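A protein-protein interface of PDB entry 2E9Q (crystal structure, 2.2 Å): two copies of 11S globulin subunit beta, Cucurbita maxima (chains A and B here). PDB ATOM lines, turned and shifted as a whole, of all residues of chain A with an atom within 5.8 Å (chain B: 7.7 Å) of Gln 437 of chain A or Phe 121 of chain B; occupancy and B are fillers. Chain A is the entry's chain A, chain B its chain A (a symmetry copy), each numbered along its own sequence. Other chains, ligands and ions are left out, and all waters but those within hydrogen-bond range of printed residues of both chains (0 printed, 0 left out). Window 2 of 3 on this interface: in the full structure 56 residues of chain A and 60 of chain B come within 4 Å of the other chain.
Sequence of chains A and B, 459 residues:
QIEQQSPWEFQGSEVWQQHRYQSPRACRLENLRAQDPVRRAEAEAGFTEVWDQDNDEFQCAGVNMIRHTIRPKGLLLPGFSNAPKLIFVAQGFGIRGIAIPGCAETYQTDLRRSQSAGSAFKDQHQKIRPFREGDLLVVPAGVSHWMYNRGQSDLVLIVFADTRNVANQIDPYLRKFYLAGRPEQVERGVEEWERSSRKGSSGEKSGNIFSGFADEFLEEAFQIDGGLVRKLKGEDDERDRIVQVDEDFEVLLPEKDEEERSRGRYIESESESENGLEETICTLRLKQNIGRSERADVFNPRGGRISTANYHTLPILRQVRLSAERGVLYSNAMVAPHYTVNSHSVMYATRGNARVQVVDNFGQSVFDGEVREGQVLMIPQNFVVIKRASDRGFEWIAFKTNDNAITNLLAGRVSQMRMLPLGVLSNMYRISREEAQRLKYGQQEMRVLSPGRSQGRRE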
ATOM      1  N   LEU A 422      -9.799   0.422  -3.800  1.00  0.00           N
ATOM      2  CA  LEU A 422      -9.650   0.466  -2.354  1.00  0.00           C
ATOM      3  C   LEU A 422     -10.780   1.286  -1.741  1.00  0.00           C
ATOM      4  O   LEU A 422     -11.274   0.961  -0.675  1.00  0.00           O
ATOM      5  CB  LEU A 422      -8.298   1.073  -1.959  1.00  0.00           C
ATOM      6  CG  LEU A 422      -7.068   0.176  -2.082  1.00  0.00           C
ATOM      7  CD1 LEU A 422      -5.842   0.952  -1.630  1.00  0.00           C
ATOM      8  CD2 LEU A 422      -7.240  -1.067  -1.222  1.00  0.00           C
ATOM      9  N   LEU A 425     -13.740  -1.031  -1.275  1.00  0.00           N
ATOM     10  CA  LEU A 425     -13.539  -1.993  -0.202  1.00  0.00           C
ATOM     11  C   LEU A 425     -13.715  -1.326   1.157  1.00  0.00           C
ATOM     12  O   LEU A 425     -14.329  -1.895   2.061  1.00  0.00           O
ATOM     13  CB  LEU A 425     -12.139  -2.585  -0.294  1.00  0.00           C
ATOM     14  CG  LEU A 425     -11.879  -3.493  -1.488  1.00  0.00           C
ATOM     15  CD1 LEU A 425     -10.384  -3.597  -1.744  1.00  0.00           C
ATOM     16  CD2 LEU A 425     -12.479  -4.862  -1.209  1.00  0.00           C
ATOM     17  N   SER A 432     -10.339   0.852   6.933  1.00  0.00           N
ATOM     18  CA  SER A 432      -9.525   1.901   6.329  1.00  0.00           C
ATOM     19  C   SER A 432      -8.726   1.401   5.133  1.00  0.00           C
ATOM     20  O   SER A 432      -8.429   0.205   5.017  1.00  0.00           O
ATOM     21  CB  SER A 432      -8.559   2.475   7.360  1.00  0.00           C
ATOM     22  OG  SER A 432      -7.710   1.454   7.844  1.00  0.00           O
ATOM     23  N   ARG A 433      -8.370   2.335   4.256  1.00  0.00           N
ATOM     24  CA  ARG A 433      -7.596   2.024   3.059  1.00  0.00           C
ATOM     25  C   ARG A 433      -6.460   1.058   3.360  1.00  0.00           C
ATOM     26  O   ARG A 433      -6.243   0.102   2.618  1.00  0.00           O
ATOM     27  CB  ARG A 433      -7.007   3.302   2.454  1.00  0.00           C
ATOM     28  CG  ARG A 433      -8.022   4.246   1.824  1.00  0.00           C
ATOM     29  CD  ARG A 433      -8.800   3.578   0.696  1.00  0.00           C
ATOM     30  NE  ARG A 433      -9.491   4.557  -0.142  1.00  0.00           N
ATOM     31  CZ  ARG A 433      -8.902   5.284  -1.087  1.00  0.00           C
ATOM     32  NH1 ARG A 433      -7.605   5.144  -1.324  1.00  0.00           N
ATOM     33  NH2 ARG A 433      -9.610   6.155  -1.791  1.00  0.00           N
ATOM     34  N   GLU A 434      -5.744   1.299   4.454  1.00  0.00           N
ATOM     35  CA  GLU A 434      -4.628   0.434   4.828  1.00  0.00           C
ATOM     36  C   GLU A 434      -5.092  -1.007   4.986  1.00  0.00           C
ATOM     37  O   GLU A 434      -4.506  -1.934   4.420  1.00  0.00           O
ATOM     38  CB  GLU A 434      -4.001   0.896   6.145  1.00  0.00           C
ATOM     39  CG  GLU A 434      -2.611   0.310   6.388  1.00  0.00           C
ATOM     40  CD  GLU A 434      -2.263   0.198   7.864  1.00  0.00           C
ATOM     41  OE1 GLU A 434      -1.058   0.071   8.188  1.00  0.00           O
ATOM     42  OE2 GLU A 434      -3.197   0.221   8.698  1.00  0.00           O
ATOM     43  N   GLU A 435      -6.146  -1.186   5.770  1.00  0.00           N
ATOM     44  CA  GLU A 435      -6.709  -2.510   6.013  1.00  0.00           C
ATOM     45  C   GLU A 435      -7.253  -3.055   4.697  1.00  0.00           C
ATOM     46  O   GLU A 435      -7.115  -4.239   4.393  1.00  0.00           O
ATOM     47  CB  GLU A 435      -7.839  -2.415   7.038  1.00  0.00           C
ATOM     48  CG  GLU A 435      -7.537  -1.521   8.237  1.00  0.00           C
ATOM     49  CD  GLU A 435      -8.711  -1.431   9.195  1.00  0.00           C
ATOM     50  OE1 GLU A 435      -9.019  -2.449   9.855  1.00  0.00           O
ATOM     51  OE2 GLU A 435      -9.336  -0.346   9.278  1.00  0.00           O
ATOM     52  N   ALA A 436      -7.876  -2.180   3.919  1.00  0.00           N
ATOM     53  CA  ALA A 436      -8.427  -2.580   2.634  1.00  0.00           C
ATOM     54  C   ALA A 436      -7.285  -3.078   1.756  1.00  0.00           C
ATOM     55  O   ALA A 436      -7.456  -3.989   0.948  1.00  0.00           O
ATOM     56  CB  ALA A 436      -9.127  -1.398   1.971  1.00  0.00           C
ATOM     57  N   GLN A 437      -6.112  -2.474   1.933  1.00  0.00           N
ATOM     58  CA  GLN A 437      -4.941  -2.851   1.160  1.00  0.00           C
ATOM     59  C   GLN A 437      -4.494  -4.233   1.588  1.00  0.00           C
ATOM     60  O   GLN A 437      -4.210  -5.087   0.753  1.00  0.00           O
ATOM     61  CB  GLN A 437      -3.807  -1.854   1.388  1.00  0.00           C
ATOM     62  CG  GLN A 437      -2.766  -1.872   0.292  1.00  0.00           C
ATOM     63  CD  GLN A 437      -1.632  -0.912   0.560  1.00  0.00           C
ATOM     64  OE1 GLN A 437      -0.938  -0.483  -0.359  1.00  0.00           O
ATOM     65  NE2 GLN A 437      -1.428  -0.578   1.827  1.00  0.00           N
ATOM     66  N   ARG A 438      -4.438  -4.450   2.897  1.00  0.00           N
ATOM     67  CA  ARG A 438      -4.034  -5.744   3.439  1.00  0.00           C
ATOM     68  C   ARG A 438      -5.048  -6.817   3.046  1.00  0.00           C
ATOM     69  O   ARG A 438      -4.704  -7.979   2.838  1.00  0.00           O
ATOM     70  CB  ARG A 438      -3.913  -5.654   4.969  1.00  0.00           C
ATOM     71  CG  ARG A 438      -3.794  -7.004   5.685  1.00  0.00           C
ATOM     72  CD  ARG A 438      -2.829  -6.938   6.884  1.00  0.00           C
ATOM     73  NE  ARG A 438      -3.254  -6.022   7.946  1.00  0.00           N
ATOM     74  CZ  ARG A 438      -4.171  -6.305   8.869  1.00  0.00           C
ATOM     75  NH1 ARG A 438      -4.774  -7.488   8.879  1.00  0.00           N
ATOM     76  NH2 ARG A 438      -4.484  -5.399   9.792  1.00  0.00           N
ATOM     77  N   LEU A 439      -6.304  -6.409   2.928  1.00  0.00           N
ATOM     78  CA  LEU A 439      -7.368  -7.333   2.575  1.00  0.00           C
ATOM     79  C   LEU A 439      -7.240  -7.820   1.129  1.00  0.00           C
ATOM     80  O   LEU A 439      -7.241  -9.029   0.880  1.00  0.00           O
ATOM     81  CB  LEU A 439      -8.724  -6.647   2.785  1.00  0.00           C
ATOM     82  CG  LEU A 439     -10.012  -7.474   2.730  1.00  0.00           C
ATOM     83  CD1 LEU A 439     -10.300  -7.909   1.307  1.00  0.00           C
ATOM     84  CD2 LEU A 439      -9.878  -8.671   3.662  1.00  0.00           C
ATOM     85  N   LYS A 440      -7.119  -6.888   0.182  1.00  0.00           N
ATOM     86  CA  LYS A 440      -7.024  -7.264  -1.231  1.00  0.00           C
ATOM     87  C   LYS A 440      -5.667  -7.705  -1.761  1.00  0.00           C
ATOM     88  O   LYS A 440      -5.606  -8.344  -2.811  1.00  0.00           O
ATOM     89  CB  LYS A 440      -7.561  -6.146  -2.131  1.00  0.00           C
ATOM     90  CG  LYS A 440      -6.677  -4.934  -2.251  1.00  0.00           C
ATOM     91  CD  LYS A 440      -7.280  -3.883  -3.194  1.00  0.00           C
ATOM     92  CE  LYS A 440      -7.272  -4.315  -4.650  1.00  0.00           C
ATOM     93  NZ  LYS A 440      -7.675  -3.183  -5.553  1.00  0.00           N
ATOM     94  N   TYR A 441      -4.581  -7.383  -1.065  1.00  0.00           N
ATOM     95  CA  TYR A 441      -3.255  -7.795  -1.544  1.00  0.00           C
ATOM     96  C   TYR A 441      -2.569  -8.762  -0.597  1.00  0.00           C
ATOM     97  O   TYR A 441      -1.408  -9.124  -0.807  1.00  0.00           O
ATOM     98  CB  TYR A 441      -2.352  -6.580  -1.751  1.00  0.00           C
ATOM     99  CG  TYR A 441      -2.899  -5.567  -2.724  1.00  0.00           C
ATOM    100  CD1 TYR A 441      -3.180  -5.918  -4.040  1.00  0.00           C
ATOM    101  CD2 TYR A 441      -3.141  -4.257  -2.326  1.00  0.00           C
ATOM    102  CE1 TYR A 441      -3.696  -4.983  -4.942  1.00  0.00           C
ATOM    103  CE2 TYR A 441      -3.656  -3.316  -3.216  1.00  0.00           C
ATOM    104  CZ  TYR A 441      -3.930  -3.686  -4.520  1.00  0.00           C
ATOM    105  OH  TYR A 441      -4.450  -2.766  -5.396  1.00  0.00           O
ATOM    106  N   GLY A 442      -3.290  -9.177   0.442  1.00  0.00           N
ATOM    107  CA  GLY A 442      -2.737 -10.094   1.422  1.00  0.00           C
ATOM    108  C   GLY A 442      -2.417 -11.468   0.868  1.00  0.00           C
ATOM    109  O   GLY A 442      -1.334 -11.993   1.099  1.00  0.00           O
ATOM    110  N   GLN B 108      -4.512   1.086 -13.179  1.00  0.00           N
ATOM    111  CA  GLN B 108      -3.745   1.674 -12.083  1.00  0.00           C
ATOM    112  C   GLN B 108      -4.137   3.133 -11.834  1.00  0.00           C
ATOM    113  O   GLN B 108      -3.890   4.000 -12.673  1.00  0.00           O
ATOM    114  CB  GLN B 108      -2.241   1.565 -12.404  1.00  0.00           C
ATOM    115  CG  GLN B 108      -1.773   0.135 -12.716  1.00  0.00           C
ATOM    116  CD  GLN B 108      -0.383   0.066 -13.363  1.00  0.00           C
ATOM    117  OE1 GLN B 108       0.140  -1.025 -13.625  1.00  0.00           O
ATOM    118  NE2 GLN B 108       0.214   1.229 -13.627  1.00  0.00           N
ATOM    119  N   THR B 109      -4.757   3.401 -10.684  1.00  0.00           N
ATOM    120  CA  THR B 109      -5.168   4.765 -10.348  1.00  0.00           C
ATOM    121  C   THR B 109      -3.958   5.593  -9.953  1.00  0.00           C
ATOM    122  O   THR B 109      -3.407   5.431  -8.857  1.00  0.00           O
ATOM    123  CB  THR B 109      -6.185   4.811  -9.180  1.00  0.00           C
ATOM    124  OG1 THR B 109      -5.867   3.794  -8.218  1.00  0.00           O
ATOM    125  CG2 THR B 109      -7.601   4.624  -9.693  1.00  0.00           C
ATOM    126  N   ASP B 110      -3.567   6.481 -10.863  1.00  0.00           N
ATOM    127  CA  ASP B 110      -2.416   7.371 -10.709  1.00  0.00           C
ATOM    128  C   ASP B 110      -2.207   7.987  -9.335  1.00  0.00           C
ATOM    129  O   ASP B 110      -3.049   7.875  -8.438  1.00  0.00           O
ATOM    130  CB  ASP B 110      -2.499   8.496 -11.742  1.00  0.00           C
ATOM    131  CG  ASP B 110      -3.756   8.412 -12.588  1.00  0.00           C
ATOM    132  OD1 ASP B 110      -3.815   7.534 -13.481  1.00  0.00           O
ATOM    133  OD2 ASP B 110      -4.685   9.217 -12.345  1.00  0.00           O
ATOM    134  N   LEU B 111      -1.067   8.661  -9.200  1.00  0.00           N
ATOM    135  CA  LEU B 111      -0.682   9.315  -7.960  1.00  0.00           C
ATOM    136  C   LEU B 111      -1.339  10.684  -7.805  1.00  0.00           C
ATOM    137  O   LEU B 111      -2.144  11.104  -8.642  1.00  0.00           O
ATOM    138  CB  LEU B 111       0.839   9.472  -7.908  1.00  0.00           C
ATOM    139  CG  LEU B 111       1.652   8.231  -8.288  1.00  0.00           C
ATOM    140  CD1 LEU B 111       3.122   8.469  -7.947  1.00  0.00           C
ATOM    141  CD2 LEU B 111       1.123   7.006  -7.547  1.00  0.00           C
ATOM    142  N   ARG B 112      -0.983  11.373  -6.726  1.00  0.00           N
ATOM    143  CA  ARG B 112      -1.520  12.697  -6.431  1.00  0.00           C
ATOM    144  C   ARG B 112      -0.389  13.707  -6.251  1.00  0.00           C
ATOM    145  O   ARG B 112       0.791  13.352  -6.298  1.00  0.00           O
ATOM    146  CB  ARG B 112      -2.380  12.644  -5.158  1.00  0.00           C
ATOM    147  CG  ARG B 112      -3.663  11.827  -5.300  1.00  0.00           C
ATOM    148  CD  ARG B 112      -4.351  11.606  -3.951  1.00  0.00           C
ATOM    149  NE  ARG B 112      -4.606  12.860  -3.238  1.00  0.00           N
ATOM    150  CZ  ARG B 112      -5.400  13.832  -3.683  1.00  0.00           C
ATOM    151  NH1 ARG B 112      -6.027  13.709  -4.848  1.00  0.00           N
ATOM    152  NH2 ARG B 112      -5.563  14.935  -2.960  1.00  0.00           N
ATOM    153  N   ALA B 120       2.967   8.356  -3.127  1.00  0.00           N
ATOM    154  CA  ALA B 120       3.111   7.911  -4.512  1.00  0.00           C
ATOM    155  C   ALA B 120       2.506   6.517  -4.731  1.00  0.00           C
ATOM    156  O   ALA B 120       3.016   5.724  -5.532  1.00  0.00           O
ATOM    157  CB  ALA B 120       4.588   7.909  -4.905  1.00  0.00           C
ATOM    158  N   PHE B 121       1.420   6.224  -4.022  1.00  0.00           N
ATOM    159  CA  PHE B 121       0.769   4.929  -4.152  1.00  0.00           C
ATOM    160  C   PHE B 121      -0.191   4.889  -5.330  1.00  0.00           C
ATOM    161  O   PHE B 121      -0.904   5.854  -5.609  1.00  0.00           O
ATOM    162  CB  PHE B 121       0.005   4.578  -2.877  1.00  0.00           C
ATOM    163  CG  PHE B 121      -0.854   3.349  -3.010  1.00  0.00           C
ATOM    164  CD1 PHE B 121      -0.282   2.112  -3.291  1.00  0.00           C
ATOM    165  CD2 PHE B 121      -2.234   3.432  -2.871  1.00  0.00           C
ATOM    166  CE1 PHE B 121      -1.072   0.971  -3.432  1.00  0.00           C
ATOM    167  CE2 PHE B 121      -3.031   2.297  -3.011  1.00  0.00           C
ATOM    168  CZ  PHE B 121      -2.448   1.064  -3.292  1.00  0.00           C
ATOM    169  N   LYS B 122      -0.201   3.756  -6.018  1.00  0.00           N
ATOM    170  CA  LYS B 122      -1.077   3.559  -7.160  1.00  0.00           C
ATOM    171  C   LYS B 122      -1.852   2.270  -6.924  1.00  0.00           C
ATOM    172  O   LYS B 122      -1.259   1.210  -6.731  1.00  0.00           O
ATOM    173  CB  LYS B 122      -0.260   3.444  -8.448  1.00  0.00           C
ATOM    174  CG  LYS B 122      -0.395   4.623  -9.405  1.00  0.00           C
ATOM    175  CD  LYS B 122       0.092   4.222 -10.789  1.00  0.00           C
ATOM    176  CE  LYS B 122      -0.295   5.245 -11.842  1.00  0.00           C
ATOM    177  NZ  LYS B 122      -0.022   4.736 -13.218  1.00  0.00           N
ATOM    178  N   ASP B 123      -3.176   2.371  -6.928  1.00  0.00           N
ATOM    179  CA  ASP B 123      -4.054   1.221  -6.717  1.00  0.00           C
ATOM    180  C   ASP B 123      -4.334   0.526  -8.052  1.00  0.00           C
ATOM    181  O   ASP B 123      -4.380   1.163  -9.103  1.00  0.00           O
ATOM    182  CB  ASP B 123      -5.371   1.701  -6.092  1.00  0.00           C
ATOM    183  CG  ASP B 123      -6.368   0.568  -5.854  1.00  0.00           C
ATOM    184  OD1 ASP B 123      -7.590   0.822  -5.981  1.00  0.00           O
ATOM    185  OD2 ASP B 123      -5.938  -0.562  -5.528  1.00  0.00           O
ATOM    186  N   GLN B 124      -4.508  -0.785  -8.012  1.00  0.00           N
ATOM    187  CA  GLN B 124      -4.812  -1.540  -9.222  1.00  0.00           C
ATOM    188  C   GLN B 124      -6.256  -2.033  -9.103  1.00  0.00           C
ATOM    189  O   GLN B 124      -6.608  -2.645  -8.103  1.00  0.00           O
ATOM    190  CB  GLN B 124      -3.853  -2.725  -9.353  1.00  0.00           C
ATOM    191  CG  GLN B 124      -3.905  -3.417 -10.696  1.00  0.00           C
ATOM    192  CD  GLN B 124      -2.671  -4.272 -10.947  1.00  0.00           C
ATOM    193  OE1 GLN B 124      -2.456  -5.289 -10.281  1.00  0.00           O
ATOM    194  NE2 GLN B 124      -1.843  -3.850 -11.904  1.00  0.00           N
ATOM    195  N   LEU B 228     -10.021  -8.600  11.167  1.00  0.00           N
ATOM    196  CA  LEU B 228     -10.478  -8.303   9.817  1.00  0.00           C
ATOM    197  C   LEU B 228     -11.609  -9.214   9.397  1.00  0.00           C
ATOM    198  O   LEU B 228     -12.530  -8.797   8.702  1.00  0.00           O
ATOM    199  CB  LEU B 228      -9.333  -8.436   8.818  1.00  0.00           C
ATOM    200  CG  LEU B 228      -8.684  -7.102   8.483  1.00  0.00           C
ATOM    201  CD1 LEU B 228      -7.602  -7.299   7.423  1.00  0.00           C
ATOM    202  CD2 LEU B 228      -9.775  -6.139   7.998  1.00  0.00           C
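Of the printed residues of chain B, Leu 422 of chain A touches Phe 121 (3.4 Å) and Asp 123 (3.1 Å).
Leu 425 of chain A touches none of the printed residues of chain B.
Of chain B, only Phe 121 comes within 4 Å of Gln 437 of chain A.
Of the printed residues of chain B, Lys 440 of chain A touches Asp 123 (3.1 Å) and Gln 124 (2.8 Å).
Asp 110 of chain B touches none of the printed residues of chain A.
Phe 121 of chain B touches just these residues of chain A: Leu 422 (3.4 Å) and Gln 437 (3.4 Å).
Printed residues of chain A within 4 Å of Gln 124 of chain B: Lys 440 (2.8 Å) and Tyr 441 (3.3 Å).
The nearest residue of chain B that does not touch Gln 437 of chain A is Lys 122 of chain B (6.6 Å).
The nearest residue of chain A that does not touch Phe 121 of chain B is Tyr 441 of chain A (4.5 Å).
Leu 422 of chain A touches Phe 121 of chain B.
CE1 of Phe 121 of chain B touches OE1 of Gln 437 of chain A, at 3.4 Å.
Arg 438 of chain A touches Leu 228 of chain B (NH1 to CD1, 3.2 Å).
The side-chain amino group (NZ) of Lys 440 of chain A is in salt-bridge range of the side-chain carboxylate (OD2) of Asp 123 of chain B (3.1 Å).
OD1 of Asp 123 of chain B is in hydrogen-bond range of N of Leu 422 of chain A (3.1 Å).
The backbone carbonyl oxygen of Gln 124 of chain B sits at hydrogen-bond distance from the side-chain amino group of Lys 440 of chain A, at 2.8 Å.
N of Gln 124 of chain B is in hydrogen-bond range of OH of Tyr 441 of chain A (3.3 Å).
OH of Tyr 441 of chain A sits at hydrogen-bond distance from OD2 of Asp 123 of chain B, 2.7 Å away.
No position is printed for both chains.
Of the 8 pairs that touch across the chains among the printed residues, none has its exchanged pair printed and touching as well.
Of the 11 printed residues of chain B, 4 touch a printed residue of chain A.
Printed residues of chain B that touch a printed residue of chain A: Phe 121, Asp 123, Gln 124 and Leu 228.
Hydrophobic or aromatic side chains of chain B that line the printed part of chain A: Phe 121 and Leu 228.
Of the 13 printed residues of chain A, 5 touch a printed residue of chain B.
Printed residues of chain A that touch a printed residue of chain B: Leu 422, Gln 437, Arg 438, Lys 440 and Tyr 441.
Hydrophobic or aromatic side chains of chain A within 4 Å of the printed part of chain B: Leu 422 and Tyr 441.
Among the printed residues, 8 pairs touch across the chains.
The backbone NH (N) of Thr 109 of chain B is in hydrogen-bond range of the backbone carbonyl oxygen (O) of Asp 123 of chain B.
OH of Tyr 441 of chain A is in hydrogen-bond range of NZ of Lys 440 of chain A.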
